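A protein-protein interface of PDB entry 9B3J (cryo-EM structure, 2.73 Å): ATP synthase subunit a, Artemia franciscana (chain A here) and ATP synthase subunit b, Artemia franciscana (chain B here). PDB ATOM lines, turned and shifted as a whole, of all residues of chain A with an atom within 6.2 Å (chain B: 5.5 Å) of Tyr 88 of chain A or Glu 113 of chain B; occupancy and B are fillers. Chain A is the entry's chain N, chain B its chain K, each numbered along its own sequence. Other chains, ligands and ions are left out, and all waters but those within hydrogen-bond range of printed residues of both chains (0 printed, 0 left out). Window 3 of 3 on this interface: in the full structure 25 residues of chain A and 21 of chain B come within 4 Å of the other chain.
Val 8 of chain A touches Glu 113 of chain B.
O of Val 109 of chain B touches OH of Tyr 88 of chain A, at 3.8 Å.
CD1 of Tyr 88 of chain A touches OE1 of Glu 113 of chain B, 3.1 Å away.
Thr 170 of chain A touches His 112 of chain B.
His 112 of chain B touches Gly 173 of chain A (CB to C, 3.5 Å).
Gly 173 of chain A touches Tyr 115 of chain B.
Of the printed residues of chain B, Val 8 of chain A touches Glu 113.
Tyr 88 of chain A touches just these residues of chain B: Tyr 108 (3.1 Å), Val 109 (3.8 Å) and Glu 113 (3.1 Å).
Printed residues of chain B within 4 Å of Thr 170 of chain A: His 112.
Printed residues of chain B within 4 Å of Gly 173 of chain A: His 112 and Tyr 115.
Printed residues of chain A within 4 Å of Val 109 of chain B: Tyr 88.
Glu 113 of chain B touches just these residues of chain A: Val 8, Pro 87 and Tyr 88.
Phe 114 of chain B touches none of the printed residues of chain A.
Of the printed residues of chain A, Tyr 115 of chain B touches Gly 173.
Gly 117 of chain B touches none of the printed residues of chain A.
The nearest printed residue of chain B that does not touch Gly 173 of chain A is Glu 111 of chain B (4.9 Å).
OH of Tyr 88 of chain A lies within hydrogen-bond range of OH of Tyr 108 of chain B (3.1 Å).
The backbone carbonyl oxygen (O) of Pro 87 of chain A sits close to the side-chain carboxylate (OE1) of Glu 113 of chain B (2.9 Å).
Hydrophobic or aromatic side chains of chain A that line the printed part of chain B: Val 8, Pro 87 and Tyr 88.
Of the 10 printed residues of chain B, 5 touch a printed residue of chain A.
Hydrophobic or aromatic side chains of chain B that line the printed part of chain A: Tyr 108, His 112 and Tyr 115.
Along chain B the printed residues that touch a printed residue of chain A span positions 108 to 115.
O of His 166 of chain A lies within hydrogen-bond range of OG1 of Thr 170 of chain A, at 2.6 Å.
The backbone carbonyl oxygen of His 112 of chain B sits at hydrogen-bond distance from the side-chain hydroxyl of Thr 116 of chain B (3.4 Å).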
ATOM      1  N   SER A   7      -8.425 -24.204 -22.269  1.00  0.00           N
ATOM      2  CA  SER A   7      -7.462 -24.261 -23.362  1.00  0.00           C
ATOM      3  C   SER A   7      -6.146 -24.917 -22.972  1.00  0.00           C
ATOM      4  O   SER A   7      -5.327 -25.188 -23.856  1.00  0.00           O
ATOM      5  CB  SER A   7      -7.197 -22.853 -23.894  1.00  0.00           C
ATOM      6  OG  SER A   7      -6.770 -21.990 -22.855  1.00  0.00           O
ATOM      7  N   VAL A   8      -5.909 -25.154 -21.679  1.00  0.00           N
ATOM      8  CA  VAL A   8      -4.746 -25.926 -21.262  1.00  0.00           C
ATOM      9  C   VAL A   8      -4.888 -27.378 -21.699  1.00  0.00           C
ATOM     10  O   VAL A   8      -3.891 -28.041 -22.012  1.00  0.00           O
ATOM     11  CB  VAL A   8      -4.556 -25.813 -19.739  1.00  0.00           C
ATOM     12  CG1 VAL A   8      -3.200 -26.353 -19.322  1.00  0.00           C
ATOM     13  CG2 VAL A   8      -4.722 -24.374 -19.298  1.00  0.00           C
ATOM     14  N   GLY A  84       4.619 -30.538 -15.390  1.00  0.00           N
ATOM     15  CA  GLY A  84       3.442 -30.029 -16.062  1.00  0.00           C
ATOM     16  C   GLY A  84       2.839 -28.801 -15.421  1.00  0.00           C
ATOM     17  O   GLY A  84       2.113 -28.061 -16.090  1.00  0.00           O
ATOM     18  N   PHE A  86       4.399 -26.159 -14.453  1.00  0.00           N
ATOM     19  CA  PHE A  86       5.015 -24.978 -15.026  1.00  0.00           C
ATOM     20  C   PHE A  86       4.140 -24.469 -16.171  1.00  0.00           C
ATOM     21  O   PHE A  86       3.460 -25.263 -16.825  1.00  0.00           O
ATOM     22  CB  PHE A  86       6.424 -25.326 -15.488  1.00  0.00           C
ATOM     23  CG  PHE A  86       7.297 -25.781 -14.373  1.00  0.00           C
ATOM     24  CD1 PHE A  86       7.280 -25.117 -13.164  1.00  0.00           C
ATOM     25  CD2 PHE A  86       8.099 -26.889 -14.507  1.00  0.00           C
ATOM     26  CE1 PHE A  86       8.068 -25.534 -12.118  1.00  0.00           C
ATOM     27  CE2 PHE A  86       8.888 -27.312 -13.459  1.00  0.00           C
ATOM     28  CZ  PHE A  86       8.872 -26.630 -12.266  1.00  0.00           C
ATOM     29  N   PRO A  87       4.121 -23.136 -16.420  1.00  0.00           N
ATOM     30  CA  PRO A  87       2.941 -22.513 -17.043  1.00  0.00           C
ATOM     31  C   PRO A  87       2.518 -23.018 -18.414  1.00  0.00           C
ATOM     32  O   PRO A  87       1.421 -23.569 -18.544  1.00  0.00           O
ATOM     33  CB  PRO A  87       3.347 -21.037 -17.125  1.00  0.00           C
ATOM     34  CG  PRO A  87       4.812 -21.042 -17.084  1.00  0.00           C
ATOM     35  CD  PRO A  87       5.163 -22.133 -16.155  1.00  0.00           C
ATOM     36  N   TYR A  88       3.368 -22.891 -19.425  1.00  0.00           N
ATOM     37  CA  TYR A  88       2.956 -23.221 -20.781  1.00  0.00           C
ATOM     38  C   TYR A  88       3.188 -24.680 -21.132  1.00  0.00           C
ATOM     39  O   TYR A  88       2.857 -25.091 -22.245  1.00  0.00           O
ATOM     40  CB  TYR A  88       3.675 -22.318 -21.783  1.00  0.00           C
ATOM     41  CG  TYR A  88       3.382 -20.856 -21.563  1.00  0.00           C
ATOM     42  CD1 TYR A  88       2.205 -20.293 -22.020  1.00  0.00           C
ATOM     43  CD2 TYR A  88       4.276 -20.043 -20.888  1.00  0.00           C
ATOM     44  CE1 TYR A  88       1.923 -18.967 -21.808  1.00  0.00           C
ATOM     45  CE2 TYR A  88       4.006 -18.713 -20.677  1.00  0.00           C
ATOM     46  CZ  TYR A  88       2.827 -18.180 -21.140  1.00  0.00           C
ATOM     47  OH  TYR A  88       2.549 -16.849 -20.936  1.00  0.00           O
ATOM     48  N   ILE A  89       3.724 -25.467 -20.208  1.00  0.00           N
ATOM     49  CA  ILE A  89       4.004 -26.876 -20.457  1.00  0.00           C
ATOM     50  C   ILE A  89       2.711 -27.670 -20.360  1.00  0.00           C
ATOM     51  O   ILE A  89       1.957 -27.538 -19.391  1.00  0.00           O
ATOM     52  CB  ILE A  89       5.050 -27.399 -19.464  1.00  0.00           C
ATOM     53  CG1 ILE A  89       6.402 -26.749 -19.729  1.00  0.00           C
ATOM     54  CG2 ILE A  89       5.177 -28.893 -19.564  1.00  0.00           C
ATOM     55  CD1 ILE A  89       7.447 -27.146 -18.733  1.00  0.00           C
ATOM     56  N   PHE A  90       2.449 -28.491 -21.372  1.00  0.00           N
ATOM     57  CA  PHE A  90       1.270 -29.342 -21.377  1.00  0.00           C
ATOM     58  C   PHE A  90       1.412 -30.463 -20.354  1.00  0.00           C
ATOM     59  O   PHE A  90       2.484 -31.055 -20.202  1.00  0.00           O
ATOM     60  CB  PHE A  90       1.061 -29.915 -22.777  1.00  0.00           C
ATOM     61  CG  PHE A  90      -0.085 -30.867 -22.883  1.00  0.00           C
ATOM     62  CD1 PHE A  90      -1.384 -30.419 -22.766  1.00  0.00           C
ATOM     63  CD2 PHE A  90       0.137 -32.207 -23.116  1.00  0.00           C
ATOM     64  CE1 PHE A  90      -2.436 -31.293 -22.865  1.00  0.00           C
ATOM     65  CE2 PHE A  90      -0.911 -33.081 -23.220  1.00  0.00           C
ATOM     66  CZ  PHE A  90      -2.198 -32.624 -23.094  1.00  0.00           C
ATOM     67  N   HIS A 166      -5.318 -27.900 -11.923  1.00  0.00           N
ATOM     68  CA  HIS A 166      -4.917 -26.835 -12.829  1.00  0.00           C
ATOM     69  C   HIS A 166      -6.060 -25.903 -13.200  1.00  0.00           C
ATOM     70  O   HIS A 166      -5.814 -24.740 -13.545  1.00  0.00           O
ATOM     71  CB  HIS A 166      -4.306 -27.414 -14.100  1.00  0.00           C
ATOM     72  CG  HIS A 166      -3.420 -26.451 -14.817  1.00  0.00           C
ATOM     73  ND1 HIS A 166      -2.073 -26.340 -14.549  1.00  0.00           N
ATOM     74  CD2 HIS A 166      -3.692 -25.528 -15.768  1.00  0.00           C
ATOM     75  CE1 HIS A 166      -1.550 -25.404 -15.318  1.00  0.00           C
ATOM     76  NE2 HIS A 166      -2.511 -24.895 -16.067  1.00  0.00           N
ATOM     77  N   THR A 170      -6.175 -21.860 -13.059  1.00  0.00           N
ATOM     78  CA  THR A 170      -6.595 -21.057 -14.202  1.00  0.00           C
ATOM     79  C   THR A 170      -7.688 -20.067 -13.824  1.00  0.00           C
ATOM     80  O   THR A 170      -7.726 -18.952 -14.363  1.00  0.00           O
ATOM     81  CB  THR A 170      -7.071 -21.965 -15.330  1.00  0.00           C
ATOM     82  OG1 THR A 170      -6.154 -23.053 -15.482  1.00  0.00           O
ATOM     83  CG2 THR A 170      -7.126 -21.203 -16.629  1.00  0.00           C
ATOM     84  N   GLY A 173      -5.845 -17.288 -12.245  1.00  0.00           N
ATOM     85  CA  GLY A 173      -5.079 -16.534 -13.224  1.00  0.00           C
ATOM     86  C   GLY A 173      -5.938 -15.603 -14.056  1.00  0.00           C
ATOM     87  O   GLY A 173      -5.510 -14.503 -14.410  1.00  0.00           O
ATOM     88  N   TYR B 108       4.153 -12.085 -26.819  1.00  0.00           N
ATOM     89  CA  TYR B 108       3.979 -12.745 -25.533  1.00  0.00           C
ATOM     90  C   TYR B 108       2.722 -12.179 -24.899  1.00  0.00           C
ATOM     91  O   TYR B 108       2.720 -11.042 -24.424  1.00  0.00           O
ATOM     92  CB  TYR B 108       5.195 -12.530 -24.637  1.00  0.00           C
ATOM     93  CG  TYR B 108       5.093 -13.229 -23.302  1.00  0.00           C
ATOM     94  CD1 TYR B 108       5.498 -14.542 -23.156  1.00  0.00           C
ATOM     95  CD2 TYR B 108       4.592 -12.574 -22.190  1.00  0.00           C
ATOM     96  CE1 TYR B 108       5.402 -15.182 -21.949  1.00  0.00           C
ATOM     97  CE2 TYR B 108       4.492 -13.207 -20.980  1.00  0.00           C
ATOM     98  CZ  TYR B 108       4.898 -14.508 -20.866  1.00  0.00           C
ATOM     99  OH  TYR B 108       4.797 -15.132 -19.650  1.00  0.00           O
ATOM    100  N   VAL B 109       1.662 -12.964 -24.879  1.00  0.00           N
ATOM    101  CA  VAL B 109       0.382 -12.514 -24.353  1.00  0.00           C
ATOM    102  C   VAL B 109       0.331 -12.797 -22.861  1.00  0.00           C
ATOM    103  O   VAL B 109       0.576 -13.927 -22.427  1.00  0.00           O
ATOM    104  CB  VAL B 109      -0.779 -13.201 -25.079  1.00  0.00           C
ATOM    105  CG1 VAL B 109      -2.088 -12.561 -24.684  1.00  0.00           C
ATOM    106  CG2 VAL B 109      -0.571 -13.122 -26.567  1.00  0.00           C
ATOM    107  N   GLU B 111      -1.350 -13.969 -20.212  1.00  0.00           N
ATOM    108  CA  GLU B 111      -2.518 -14.800 -19.999  1.00  0.00           C
ATOM    109  C   GLU B 111      -2.609 -15.204 -18.534  1.00  0.00           C
ATOM    110  O   GLU B 111      -1.879 -14.701 -17.676  1.00  0.00           O
ATOM    111  CB  GLU B 111      -2.469 -16.023 -20.914  1.00  0.00           C
ATOM    112  CG  GLU B 111      -2.856 -15.737 -22.349  1.00  0.00           C
ATOM    113  CD  GLU B 111      -3.627 -16.879 -22.976  1.00  0.00           C
ATOM    114  OE1 GLU B 111      -3.753 -17.937 -22.326  1.00  0.00           O
ATOM    115  OE2 GLU B 111      -4.116 -16.715 -24.111  1.00  0.00           O
ATOM    116  N   HIS B 112      -3.518 -16.133 -18.239  1.00  0.00           N
ATOM    117  CA  HIS B 112      -3.681 -16.660 -16.892  1.00  0.00           C
ATOM    118  C   HIS B 112      -2.502 -17.504 -16.434  1.00  0.00           C
ATOM    119  O   HIS B 112      -2.434 -17.844 -15.248  1.00  0.00           O
ATOM    120  CB  HIS B 112      -4.966 -17.485 -16.808  1.00  0.00           C
ATOM    121  CG  HIS B 112      -5.158 -18.421 -17.959  1.00  0.00           C
ATOM    122  ND1 HIS B 112      -4.391 -19.551 -18.135  1.00  0.00           N
ATOM    123  CD2 HIS B 112      -6.032 -18.393 -18.992  1.00  0.00           C
ATOM    124  CE1 HIS B 112      -4.783 -20.180 -19.229  1.00  0.00           C
ATOM    125  NE2 HIS B 112      -5.777 -19.498 -19.768  1.00  0.00           N
ATOM    126  N   GLU B 113      -1.588 -17.862 -17.333  1.00  0.00           N
ATOM    127  CA  GLU B 113      -0.422 -18.652 -16.973  1.00  0.00           C
ATOM    128  C   GLU B 113       0.810 -17.812 -16.687  1.00  0.00           C
ATOM    129  O   GLU B 113       1.780 -18.341 -16.140  1.00  0.00           O
ATOM    130  CB  GLU B 113      -0.108 -19.658 -18.083  1.00  0.00           C
ATOM    131  CG  GLU B 113      -1.177 -20.722 -18.225  1.00  0.00           C
ATOM    132  CD  GLU B 113      -0.883 -21.688 -19.343  1.00  0.00           C
ATOM    133  OE1 GLU B 113       0.131 -21.488 -20.033  1.00  0.00           O
ATOM    134  OE2 GLU B 113      -1.658 -22.649 -19.529  1.00  0.00           O
ATOM    135  N   PHE B 114       0.801 -16.529 -17.041  1.00  0.00           N
ATOM    136  CA  PHE B 114       1.920 -15.665 -16.688  1.00  0.00           C
ATOM    137  C   PHE B 114       2.015 -15.478 -15.181  1.00  0.00           C
ATOM    138  O   PHE B 114       3.115 -15.445 -14.623  1.00  0.00           O
ATOM    139  CB  PHE B 114       1.783 -14.320 -17.392  1.00  0.00           C
ATOM    140  CG  PHE B 114       2.694 -13.260 -16.860  1.00  0.00           C
ATOM    141  CD1 PHE B 114       4.039 -13.276 -17.158  1.00  0.00           C
ATOM    142  CD2 PHE B 114       2.200 -12.234 -16.072  1.00  0.00           C
ATOM    143  CE1 PHE B 114       4.878 -12.296 -16.673  1.00  0.00           C
ATOM    144  CE2 PHE B 114       3.034 -11.255 -15.586  1.00  0.00           C
ATOM    145  CZ  PHE B 114       4.374 -11.287 -15.886  1.00  0.00           C
ATOM    146  N   TYR B 115       0.871 -15.356 -14.506  1.00  0.00           N
ATOM    147  CA  TYR B 115       0.878 -15.216 -13.054  1.00  0.00           C
ATOM    148  C   TYR B 115       1.178 -16.537 -12.365  1.00  0.00           C
ATOM    149  O   TYR B 115       1.720 -16.548 -11.254  1.00  0.00           O
ATOM    150  CB  TYR B 115      -0.455 -14.648 -12.589  1.00  0.00           C
ATOM    151  CG  TYR B 115      -0.829 -13.416 -13.358  1.00  0.00           C
ATOM    152  CD1 TYR B 115      -0.204 -12.207 -13.105  1.00  0.00           C
ATOM    153  CD2 TYR B 115      -1.781 -13.465 -14.356  1.00  0.00           C
ATOM    154  CE1 TYR B 115      -0.528 -11.080 -13.816  1.00  0.00           C
ATOM    155  CE2 TYR B 115      -2.113 -12.344 -15.071  1.00  0.00           C
ATOM    156  CZ  TYR B 115      -1.485 -11.154 -14.798  1.00  0.00           C
ATOM    157  OH  TYR B 115      -1.823 -10.034 -15.514  1.00  0.00           O
ATOM    158  N   THR B 116       0.858 -17.658 -13.012  1.00  0.00           N
ATOM    159  CA  THR B 116       1.344 -18.945 -12.531  1.00  0.00           C
ATOM    160  C   THR B 116       2.859 -19.028 -12.641  1.00  0.00           C
ATOM    161  O   THR B 116       3.529 -19.509 -11.720  1.00  0.00           O
ATOM    162  CB  THR B 116       0.681 -20.078 -13.309  1.00  0.00           C
ATOM    163  OG1 THR B 116      -0.741 -19.962 -13.195  1.00  0.00           O
ATOM    164  CG2 THR B 116       1.103 -21.420 -12.758  1.00  0.00           C
ATOM    165  N   GLY B 117       3.420 -18.540 -13.747  1.00  0.00           N
ATOM    166  CA  GLY B 117       4.865 -18.523 -13.888  1.00  0.00           C
ATOM    167  C   GLY B 117       5.544 -17.590 -12.912  1.00  0.00           C
ATOM    168  O   GLY B 117       6.637 -17.885 -12.422  1.00  0.00           O
ATOM    169  N   VAL B 118       4.905 -16.464 -12.600  1.00  0.00           N
ATOM    170  CA  VAL B 118       5.454 -15.532 -11.619  1.00  0.00           C
ATOM    171  C   VAL B 118       5.449 -16.156 -10.229  1.00  0.00           C
ATOM    172  O   VAL B 118       6.443 -16.083  -9.497  1.00  0.00           O
ATOM    173  CB  VAL B 118       4.677 -14.206 -11.654  1.00  0.00           C
ATOM    174  CG1 VAL B 118       4.927 -13.392 -10.400  1.00  0.00           C
ATOM    175  CG2 VAL B 118       5.067 -13.409 -12.883  1.00  0.00           C
